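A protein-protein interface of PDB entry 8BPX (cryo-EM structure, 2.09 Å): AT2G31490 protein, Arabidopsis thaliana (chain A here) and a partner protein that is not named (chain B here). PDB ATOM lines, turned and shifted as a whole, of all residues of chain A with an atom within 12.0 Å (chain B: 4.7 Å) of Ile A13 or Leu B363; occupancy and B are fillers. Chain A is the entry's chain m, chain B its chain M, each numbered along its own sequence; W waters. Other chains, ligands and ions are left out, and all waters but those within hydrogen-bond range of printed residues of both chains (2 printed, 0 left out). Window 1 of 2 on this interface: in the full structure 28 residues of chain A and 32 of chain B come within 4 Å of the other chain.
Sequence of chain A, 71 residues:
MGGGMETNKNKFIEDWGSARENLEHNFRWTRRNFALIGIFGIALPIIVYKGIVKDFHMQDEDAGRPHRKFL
The side-chain hydroxyl (OH) of Tyr B366 is in hydrogen-bond range of the backbone NH (N) of Asn A10.
OH of Tyr B366 lies within hydrogen-bond range of OE1 of Glu A14, at 3.0 Å.
The backbone carbonyl oxygen of Phe B445 is in hydrogen-bond range of the backbone NH of Asn A8, 3.0 Å away.
The side-chain hydroxyl of Tyr B367 is in hydrogen-bond range of the backbone carbonyl oxygen of Thr B361 (2.8 Å).
The backbone NH (N) of Val B364 sits at hydrogen-bond distance from the backbone carbonyl oxygen (O) of Ile B302 (3.1 Å).
The side-chain amide oxygen of Asn A10 lies within hydrogen-bond range of the backbone NH of Ile A13.
OD1 of Asn A10 sits at hydrogen-bond distance from N of Phe A12, at 3.0 Å.
The backbone carbonyl oxygen (O) of Glu A14 sits at hydrogen-bond distance from the side-chain hydroxyl (OG) of Ser A18, at 2.7 Å.
The backbone NH (N) of Leu B363 lies within hydrogen-bond range of the side-chain hydroxyl (OG1) of Thr B361.
Thr A7 touches Thr B361 (CG2 to CG2, 3.6 Å).
Thr A7 touches Tyr B366.
Phe B445 touches Thr A7.
Lys A9 touches Thr B361 (NZ to CB, 3.8 Å).
CA of Lys A9 touches OH of Tyr B366, 3.7 Å away.
CG2 of Ile A13 touches CD1 of Leu B363, 3.7 Å away.
Ile A13 touches Tyr B366.
CD1 of Ile A13 touches CZ of Phe B445 (3.8 Å).
Trp A16 touches Ile B302.
Ile B302 touches Arg A20.
Of chain B, only Leu B363, Arg B365, Tyr B366 and Phe B445 come within 4 Å of Ile A13.
Printed residues of chain B within 4 Å of Glu A14: Tyr B366.
Printed residues of chain B within 4 Å of Trp A16: Ile B302 (3.4 Å).
Ser A18 touches none of the printed residues of chain B.
Of the printed residues of chain B, Arg A20 touches Ile B302 (3.6 Å).
Of the printed residues of chain A, Ile B302 touches Trp A16 (3.4 Å) and Arg A20 (3.6 Å).
Leu B363 touches just one residue of chain A: Ile A13 (3.7 Å).
Of chain A, only Ile A13 comes within 4 Å of Arg B365.
No residue of chain A comes within 4 Å of Tyr B367.
The nearest printed residue of chain B that does not touch Ile A13 is Ile B302 (6.2 Å).
The nearest residue of chain A that does not touch Leu B363 is Glu A14 (4.3 Å).
Of the 18 printed residues of chain A, 8 touch a printed residue of chain B.
Printed residues of chain A that touch a printed residue of chain B: Thr A7, Asn A8, Lys A9, Asn A10, Ile A13, Glu A14, Trp A16 and Arg A20.
Of the 9 printed residues of chain B, 6 touch a printed residue of chain A.
Hydrophobic or aromatic side chains of chain B within 4 Å of the printed part of chain A: Ile B302, Leu B363, Tyr B366 and Phe B445.
Among the printed residues, no Asp or Glu carboxylate lies within 4 Å of a Lys or Arg side-chain nitrogen of the other chain.
Water W1 bridges the side-chain hydroxyl of Thr B361 and the side-chain carboxylate of Glu A14.
Water W2 bridges the backbone carbonyl oxygen (O) of Phe B445 (3.1 Å) and the side-chain amide oxygen (OD1) of Asn A8 (3.4 Å).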
ATOM      1  N   MET A   5     -10.458  19.175   7.831  1.00  0.00           N
ATOM      2  CA  MET A   5     -10.544  20.099   8.983  1.00  0.00           C
ATOM      3  C   MET A   5     -11.647  19.596   9.922  1.00  0.00           C
ATOM      4  O   MET A   5     -11.625  19.994  11.062  1.00  0.00           O
ATOM      5  CB  MET A   5     -10.831  21.527   8.514  1.00  0.00           C
ATOM      6  CG  MET A   5      -9.718  22.216   7.795  1.00  0.00           C
ATOM      7  SD  MET A   5     -10.208  23.902   7.345  1.00  0.00           S
ATOM      8  CE  MET A   5      -9.538  24.798   8.744  1.00  0.00           C
ATOM      9  N   GLU A   6     -12.565  18.727   9.464  1.00  0.00           N
ATOM     10  CA  GLU A   6     -13.630  18.317  10.369  1.00  0.00           C
ATOM     11  C   GLU A   6     -13.059  17.617  11.594  1.00  0.00           C
ATOM     12  O   GLU A   6     -12.038  16.929  11.518  1.00  0.00           O
ATOM     13  CB  GLU A   6     -14.615  17.395   9.645  1.00  0.00           C
ATOM     14  CG  GLU A   6     -15.606  18.132   8.776  1.00  0.00           C
ATOM     15  CD  GLU A   6     -16.766  17.260   8.329  1.00  0.00           C
ATOM     16  OE1 GLU A   6     -16.957  17.108   7.103  1.00  0.00           O
ATOM     17  OE2 GLU A   6     -17.485  16.728   9.200  1.00  0.00           O
ATOM     18  N   THR A   7     -13.710  17.821  12.733  1.00  0.00           N
ATOM     19  CA  THR A   7     -13.276  17.171  13.958  1.00  0.00           C
ATOM     20  C   THR A   7     -13.443  15.664  13.853  1.00  0.00           C
ATOM     21  O   THR A   7     -14.382  15.155  13.235  1.00  0.00           O
ATOM     22  CB  THR A   7     -14.057  17.695  15.168  1.00  0.00           C
ATOM     23  OG1 THR A   7     -13.814  16.852  16.301  1.00  0.00           O
ATOM     24  CG2 THR A   7     -15.517  17.703  14.884  1.00  0.00           C
ATOM     25  N   ASN A   8     -12.505  14.948  14.458  1.00  0.00           N
ATOM     26  CA  ASN A   8     -12.620  13.504  14.590  1.00  0.00           C
ATOM     27  C   ASN A   8     -13.496  13.218  15.800  1.00  0.00           C
ATOM     28  O   ASN A   8     -13.078  13.425  16.943  1.00  0.00           O
ATOM     29  CB  ASN A   8     -11.241  12.871  14.718  1.00  0.00           C
ATOM     30  CG  ASN A   8     -10.540  12.764  13.390  1.00  0.00           C
ATOM     31  OD1 ASN A   8      -9.547  13.441  13.144  1.00  0.00           O
ATOM     32  ND2 ASN A   8     -11.065  11.923  12.514  1.00  0.00           N
ATOM     33  N   LYS A   9     -14.719  12.767  15.540  1.00  0.00           N
ATOM     34  CA  LYS A   9     -15.696  12.568  16.600  1.00  0.00           C
ATOM     35  C   LYS A   9     -15.221  11.507  17.584  1.00  0.00           C
ATOM     36  O   LYS A   9     -14.584  10.522  17.204  1.00  0.00           O
ATOM     37  CB  LYS A   9     -17.036  12.145  16.001  1.00  0.00           C
ATOM     38  CG  LYS A   9     -18.126  13.187  16.020  1.00  0.00           C
ATOM     39  CD  LYS A   9     -17.647  14.570  15.648  1.00  0.00           C
ATOM     40  CE  LYS A   9     -18.835  15.406  15.189  1.00  0.00           C
ATOM     41  NZ  LYS A   9     -18.476  16.696  14.558  1.00  0.00           N
ATOM     42  N   ASN A  10     -15.523  11.726  18.856  1.00  0.00           N
ATOM     43  CA  ASN A  10     -15.356  10.729  19.902  1.00  0.00           C
ATOM     44  C   ASN A  10     -16.739  10.260  20.332  1.00  0.00           C
ATOM     45  O   ASN A  10     -17.606  11.084  20.639  1.00  0.00           O
ATOM     46  CB  ASN A  10     -14.583  11.296  21.093  1.00  0.00           C
ATOM     47  CG  ASN A  10     -14.564  10.356  22.281  1.00  0.00           C
ATOM     48  OD1 ASN A  10     -15.470  10.364  23.110  1.00  0.00           O
ATOM     49  ND2 ASN A  10     -13.518   9.549  22.378  1.00  0.00           N
ATOM     50  N   LYS A  11     -16.938   8.942  20.357  1.00  0.00           N
ATOM     51  CA  LYS A  11     -18.276   8.395  20.567  1.00  0.00           C
ATOM     52  C   LYS A  11     -18.826   8.764  21.940  1.00  0.00           C
ATOM     53  O   LYS A  11     -20.018   9.051  22.082  1.00  0.00           O
ATOM     54  CB  LYS A  11     -18.255   6.878  20.371  1.00  0.00           C
ATOM     55  CG  LYS A  11     -19.199   6.099  21.266  1.00  0.00           C
ATOM     56  CD  LYS A  11     -19.366   4.666  20.769  1.00  0.00           C
ATOM     57  CE  LYS A  11     -19.630   3.704  21.912  1.00  0.00           C
ATOM     58  NZ  LYS A  11     -18.539   3.732  22.921  1.00  0.00           N
ATOM     59  N   PHE A  12     -17.973   8.768  22.962  1.00  0.00           N
ATOM     60  CA  PHE A  12     -18.434   9.090  24.308  1.00  0.00           C
ATOM     61  C   PHE A  12     -18.789  10.567  24.446  1.00  0.00           C
ATOM     62  O   PHE A  12     -19.757  10.915  25.128  1.00  0.00           O
ATOM     63  CB  PHE A  12     -17.372   8.685  25.321  1.00  0.00           C
ATOM     64  CG  PHE A  12     -16.982   7.243  25.229  1.00  0.00           C
ATOM     65  CD1 PHE A  12     -17.701   6.278  25.909  1.00  0.00           C
ATOM     66  CD2 PHE A  12     -15.913   6.847  24.440  1.00  0.00           C
ATOM     67  CE1 PHE A  12     -17.349   4.949  25.828  1.00  0.00           C
ATOM     68  CE2 PHE A  12     -15.560   5.516  24.353  1.00  0.00           C
ATOM     69  CZ  PHE A  12     -16.282   4.568  25.044  1.00  0.00           C
ATOM     70  N   ILE A  13     -18.021  11.446  23.799  1.00  0.00           N
ATOM     71  CA  ILE A  13     -18.322  12.874  23.831  1.00  0.00           C
ATOM     72  C   ILE A  13     -19.653  13.157  23.143  1.00  0.00           C
ATOM     73  O   ILE A  13     -20.479  13.933  23.642  1.00  0.00           O
ATOM     74  CB  ILE A  13     -17.165  13.666  23.196  1.00  0.00           C
ATOM     75  CG1 ILE A  13     -15.918  13.567  24.076  1.00  0.00           C
ATOM     76  CG2 ILE A  13     -17.545  15.118  22.996  1.00  0.00           C
ATOM     77  CD1 ILE A  13     -14.676  14.113  23.421  1.00  0.00           C
ATOM     78  N   GLU A  14     -19.893  12.517  21.998  1.00  0.00           N
ATOM     79  CA  GLU A  14     -21.172  12.684  21.317  1.00  0.00           C
ATOM     80  C   GLU A  14     -22.323  12.074  22.108  1.00  0.00           C
ATOM     81  O   GLU A  14     -23.425  12.631  22.123  1.00  0.00           O
ATOM     82  CB  GLU A  14     -21.097  12.101  19.909  1.00  0.00           C
ATOM     83  CG  GLU A  14     -19.976  12.705  19.110  1.00  0.00           C
ATOM     84  CD  GLU A  14     -20.346  14.071  18.565  1.00  0.00           C
ATOM     85  OE1 GLU A  14     -19.434  14.862  18.263  1.00  0.00           O
ATOM     86  OE2 GLU A  14     -21.556  14.356  18.441  1.00  0.00           O
ATOM     87  N   ASP A  15     -22.092  10.936  22.770  1.00  0.00           N
ATOM     88  CA  ASP A  15     -23.124  10.370  23.635  1.00  0.00           C
ATOM     89  C   ASP A  15     -23.477  11.327  24.763  1.00  0.00           C
ATOM     90  O   ASP A  15     -24.654  11.531  25.070  1.00  0.00           O
ATOM     91  CB  ASP A  15     -22.660   9.030  24.208  1.00  0.00           C
ATOM     92  CG  ASP A  15     -22.711   7.919  23.195  1.00  0.00           C
ATOM     93  OD1 ASP A  15     -21.957   6.937  23.343  1.00  0.00           O
ATOM     94  OD2 ASP A  15     -23.503   8.033  22.238  1.00  0.00           O
ATOM     95  N   TRP A  16     -22.460  11.928  25.382  1.00  0.00           N
ATOM     96  CA  TRP A  16     -22.668  12.921  26.430  1.00  0.00           C
ATOM     97  C   TRP A  16     -23.477  14.110  25.915  1.00  0.00           C
ATOM     98  O   TRP A  16     -24.455  14.535  26.548  1.00  0.00           O
ATOM     99  CB  TRP A  16     -21.296  13.352  26.942  1.00  0.00           C
ATOM    100  CG  TRP A  16     -21.233  14.366  28.024  1.00  0.00           C
ATOM    101  CD1 TRP A  16     -21.735  14.262  29.285  1.00  0.00           C
ATOM    102  CD2 TRP A  16     -20.592  15.638  27.947  1.00  0.00           C
ATOM    103  NE1 TRP A  16     -21.448  15.397  30.000  1.00  0.00           N
ATOM    104  CE2 TRP A  16     -20.747  16.258  29.199  1.00  0.00           C
ATOM    105  CE3 TRP A  16     -19.903  16.315  26.936  1.00  0.00           C
ATOM    106  CZ2 TRP A  16     -20.242  17.528  29.468  1.00  0.00           C
ATOM    107  CZ3 TRP A  16     -19.401  17.569  27.205  1.00  0.00           C
ATOM    108  CH2 TRP A  16     -19.572  18.162  28.461  1.00  0.00           C
ATOM    109  N   GLY A  17     -23.109  14.629  24.742  1.00  0.00           N
ATOM    110  CA  GLY A  17     -23.843  15.751  24.173  1.00  0.00           C
ATOM    111  C   GLY A  17     -25.291  15.423  23.853  1.00  0.00           C
ATOM    112  O   GLY A  17     -26.200  16.193  24.184  1.00  0.00           O
ATOM    113  N   SER A  18     -25.529  14.274  23.217  1.00  0.00           N
ATOM    114  CA  SER A  18     -26.895  13.894  22.869  1.00  0.00           C
ATOM    115  C   SER A  18     -27.731  13.604  24.108  1.00  0.00           C
ATOM    116  O   SER A  18     -28.929  13.901  24.125  1.00  0.00           O
ATOM    117  CB  SER A  18     -26.892  12.691  21.926  1.00  0.00           C
ATOM    118  OG  SER A  18     -25.991  11.690  22.353  1.00  0.00           O
ATOM    119  N   ALA A  19     -27.125  13.034  25.152  1.00  0.00           N
ATOM    120  CA  ALA A  19     -27.838  12.868  26.414  1.00  0.00           C
ATOM    121  C   ALA A  19     -28.239  14.219  26.987  1.00  0.00           C
ATOM    122  O   ALA A  19     -29.345  14.372  27.518  1.00  0.00           O
ATOM    123  CB  ALA A  19     -26.976  12.097  27.411  1.00  0.00           C
ATOM    124  N   ARG A  20     -27.363  15.215  26.833  1.00  0.00           N
ATOM    125  CA  ARG A  20     -27.691  16.590  27.296  1.00  0.00           C
ATOM    126  C   ARG A  20     -28.882  17.122  26.491  1.00  0.00           C
ATOM    127  O   ARG A  20     -29.760  17.764  27.102  1.00  0.00           O
ATOM    128  CB  ARG A  20     -26.470  17.503  27.155  1.00  0.00           C
ATOM    129  CG  ARG A  20     -26.688  18.926  27.648  1.00  0.00           C
ATOM    130  CD  ARG A  20     -27.128  18.995  29.099  1.00  0.00           C
ATOM    131  NE  ARG A  20     -26.194  18.344  30.010  1.00  0.00           N
ATOM    132  CZ  ARG A  20     -25.111  18.913  30.532  1.00  0.00           C
ATOM    133  NH1 ARG A  20     -24.802  20.163  30.236  1.00  0.00           N
ATOM    134  NH2 ARG A  20     -24.337  18.221  31.345  1.00  0.00           N
ATOM    135  N   GLU A  21     -28.922  16.853  25.180  1.00  0.00           N
ATOM    136  CA  GLU A  21     -29.991  17.401  24.349  1.00  0.00           C
ATOM    137  C   GLU A  21     -31.349  16.734  24.563  1.00  0.00           C
ATOM    138  O   GLU A  21     -32.353  17.262  24.076  1.00  0.00           O
ATOM    139  CB  GLU A  21     -29.634  17.304  22.860  1.00  0.00           C
ATOM    140  CG  GLU A  21     -28.333  17.958  22.475  1.00  0.00           C
ATOM    141  CD  GLU A  21     -27.546  17.144  21.466  1.00  0.00           C
ATOM    142  OE1 GLU A  21     -26.370  17.477  21.225  1.00  0.00           O
ATOM    143  OE2 GLU A  21     -28.101  16.175  20.911  1.00  0.00           O
ATOM    144  N   ASN A  22     -31.422  15.610  25.266  1.00  0.00           N
ATOM    145  CA  ASN A  22     -32.660  14.849  25.375  1.00  0.00           C
ATOM    146  C   ASN A  22     -33.046  14.598  26.827  1.00  0.00           C
ATOM    147  O   ASN A  22     -33.568  13.541  27.179  1.00  0.00           O
ATOM    148  CB  ASN A  22     -32.545  13.537  24.606  1.00  0.00           C
ATOM    149  CG  ASN A  22     -32.249  13.755  23.140  1.00  0.00           C
ATOM    150  OD1 ASN A  22     -31.246  13.281  22.617  1.00  0.00           O
ATOM    151  ND2 ASN A  22     -33.120  14.494  22.472  1.00  0.00           N
ATOM    152  N   ILE B 302     -22.996  23.136  27.303  1.00  0.00           N
ATOM    153  CA  ILE B 302     -21.789  22.565  26.719  1.00  0.00           C
ATOM    154  C   ILE B 302     -21.687  22.799  25.222  1.00  0.00           C
ATOM    155  O   ILE B 302     -20.739  22.320  24.597  1.00  0.00           O
ATOM    156  CB  ILE B 302     -21.675  21.059  27.034  1.00  0.00           C
ATOM    157  CG1 ILE B 302     -22.796  20.284  26.336  1.00  0.00           C
ATOM    158  CG2 ILE B 302     -21.698  20.833  28.530  1.00  0.00           C
ATOM    159  CD1 ILE B 302     -22.778  18.812  26.601  1.00  0.00           C
ATOM    160  N   THR B 361     -18.515  21.119  14.530  1.00  0.00           N
ATOM    161  CA  THR B 361     -18.942  20.695  15.854  1.00  0.00           C
ATOM    162  C   THR B 361     -19.248  21.927  16.689  1.00  0.00           C
ATOM    163  O   THR B 361     -18.615  22.975  16.538  1.00  0.00           O
ATOM    164  CB  THR B 361     -17.893  19.833  16.572  1.00  0.00           C
ATOM    165  OG1 THR B 361     -18.361  19.522  17.888  1.00  0.00           O
ATOM    166  CG2 THR B 361     -16.569  20.577  16.689  1.00  0.00           C
ATOM    167  N   ARG B 362     -20.230  21.792  17.570  1.00  0.00           N
ATOM    168  CA  ARG B 362     -20.589  22.848  18.499  1.00  0.00           C
ATOM    169  C   ARG B 362     -20.186  22.511  19.926  1.00  0.00           C
ATOM    170  O   ARG B 362     -20.354  23.347  20.820  1.00  0.00           O
ATOM    171  CB  ARG B 362     -22.094  23.122  18.433  1.00  0.00           C
ATOM    172  CG  ARG B 362     -22.552  23.739  17.120  1.00  0.00           C
ATOM    173  CD  ARG B 362     -23.993  24.218  17.184  1.00  0.00           C
ATOM    174  NE  ARG B 362     -24.917  23.164  17.581  1.00  0.00           N
ATOM    175  CZ  ARG B 362     -26.003  22.825  16.901  1.00  0.00           C
ATOM    176  NH1 ARG B 362     -26.320  23.421  15.765  1.00  0.00           N
ATOM    177  NH2 ARG B 362     -26.788  21.861  17.372  1.00  0.00           N
ATOM    178  N   LEU B 363     -19.652  21.318  20.154  1.00  0.00           N
ATOM    179  CA  LEU B 363     -19.312  20.867  21.494  1.00  0.00           C
ATOM    180  C   LEU B 363     -18.015  21.530  21.941  1.00  0.00           C
ATOM    181  O   LEU B 363     -16.993  21.435  21.255  1.00  0.00           O
ATOM    182  CB  LEU B 363     -19.189  19.344  21.505  1.00  0.00           C
ATOM    183  CG  LEU B 363     -20.531  18.599  21.468  1.00  0.00           C
ATOM    184  CD1 LEU B 363     -20.381  17.127  21.789  1.00  0.00           C
ATOM    185  CD2 LEU B 363     -21.542  19.247  22.402  1.00  0.00           C
ATOM    186  N   VAL B 364     -18.063  22.199  23.094  1.00  0.00           N
ATOM    187  CA  VAL B 364     -16.924  22.979  23.570  1.00  0.00           C
ATOM    188  C   VAL B 364     -15.707  22.093  23.806  1.00  0.00           C
ATOM    189  O   VAL B 364     -14.570  22.519  23.576  1.00  0.00           O
ATOM    190  CB  VAL B 364     -17.318  23.768  24.840  1.00  0.00           C
ATOM    191  CG1 VAL B 364     -16.115  24.483  25.442  1.00  0.00           C
ATOM    192  CG2 VAL B 364     -18.420  24.768  24.532  1.00  0.00           C
ATOM    193  N   ARG B 365     -15.918  20.845  24.235  1.00  0.00           N
ATOM    194  CA  ARG B 365     -14.793  20.002  24.632  1.00  0.00           C
ATOM    195  C   ARG B 365     -13.821  19.739  23.486  1.00  0.00           C
ATOM    196  O   ARG B 365     -12.632  19.517  23.730  1.00  0.00           O
ATOM    197  CB  ARG B 365     -15.271  18.667  25.198  1.00  0.00           C
ATOM    198  CG  ARG B 365     -14.969  18.547  26.670  1.00  0.00           C
ATOM    199  CD  ARG B 365     -13.537  18.105  26.918  1.00  0.00           C
ATOM    200  NE  ARG B 365     -13.128  16.916  26.186  1.00  0.00           N
ATOM    201  CZ  ARG B 365     -13.049  15.704  26.719  1.00  0.00           C
ATOM    202  NH1 ARG B 365     -13.353  15.484  27.987  1.00  0.00           N
ATOM    203  NH2 ARG B 365     -12.635  14.692  25.966  1.00  0.00           N
ATOM    204  N   TYR B 366     -14.296  19.748  22.240  1.00  0.00           N
ATOM    205  CA  TYR B 366     -13.404  19.462  21.121  1.00  0.00           C
ATOM    206  C   TYR B 366     -12.409  20.589  20.880  1.00  0.00           C
ATOM    207  O   TYR B 366     -11.300  20.339  20.399  1.00  0.00           O
ATOM    208  CB  TYR B 366     -14.205  19.206  19.847  1.00  0.00           C
ATOM    209  CG  TYR B 366     -14.906  17.875  19.799  1.00  0.00           C
ATOM    210  CD1 TYR B 366     -14.212  16.688  20.005  1.00  0.00           C
ATOM    211  CD2 TYR B 366     -16.264  17.803  19.533  1.00  0.00           C
ATOM    212  CE1 TYR B 366     -14.858  15.470  19.952  1.00  0.00           C
ATOM    213  CE2 TYR B 366     -16.919  16.597  19.477  1.00  0.00           C
ATOM    214  CZ  TYR B 366     -16.216  15.433  19.684  1.00  0.00           C
ATOM    215  OH  TYR B 366     -16.881  14.234  19.626  1.00  0.00           O
ATOM    216  N   TYR B 367     -12.782  21.827  21.192  1.00  0.00           N
ATOM    217  CA  TYR B 367     -11.932  22.967  20.909  1.00  0.00           C
ATOM    218  C   TYR B 367     -10.951  23.194  22.058  1.00  0.00           C
ATOM    219  O   TYR B 367     -10.913  22.451  23.038  1.00  0.00           O
ATOM    220  CB  TYR B 367     -12.776  24.210  20.643  1.00  0.00           C
ATOM    221  CG  TYR B 367     -13.646  24.130  19.411  1.00  0.00           C
ATOM    222  CD1 TYR B 367     -13.113  24.334  18.147  1.00  0.00           C
ATOM    223  CD2 TYR B 367     -15.005  23.863  19.514  1.00  0.00           C
ATOM    224  CE1 TYR B 367     -13.902  24.271  17.024  1.00  0.00           C
ATOM    225  CE2 TYR B 367     -15.805  23.795  18.393  1.00  0.00           C
ATOM    226  CZ  TYR B 367     -15.251  24.000  17.151  1.00  0.00           C
ATOM    227  OH  TYR B 367     -16.044  23.933  16.032  1.00  0.00           O
ATOM    228  N   PHE B 445      -8.525  15.551  18.149  1.00  0.00           N
ATOM    229  CA  PHE B 445      -9.797  16.037  17.630  1.00  0.00           C
ATOM    230  C   PHE B 445      -9.622  16.958  16.432  1.00  0.00           C
ATOM    231  O   PHE B 445     -10.244  16.747  15.390  1.00  0.00           O
ATOM    232  CB  PHE B 445     -10.599  16.763  18.716  1.00  0.00           C
ATOM    233  CG  PHE B 445     -10.739  15.996  19.991  1.00  0.00           C
ATOM    234  CD1 PHE B 445     -11.070  14.650  19.974  1.00  0.00           C
ATOM    235  CD2 PHE B 445     -10.591  16.629  21.211  1.00  0.00           C
ATOM    236  CE1 PHE B 445     -11.212  13.949  21.147  1.00  0.00           C
ATOM    237  CE2 PHE B 445     -10.738  15.930  22.388  1.00  0.00           C
ATOM    238  CZ  PHE B 445     -11.049  14.591  22.356  1.00  0.00           C
HETATM  239  O   HOH W   1     -20.020  17.591  17.615  1.00  0.00           O
HETATM  240  O   HOH W   2      -7.458  15.872  14.330  1.00  0.00           O
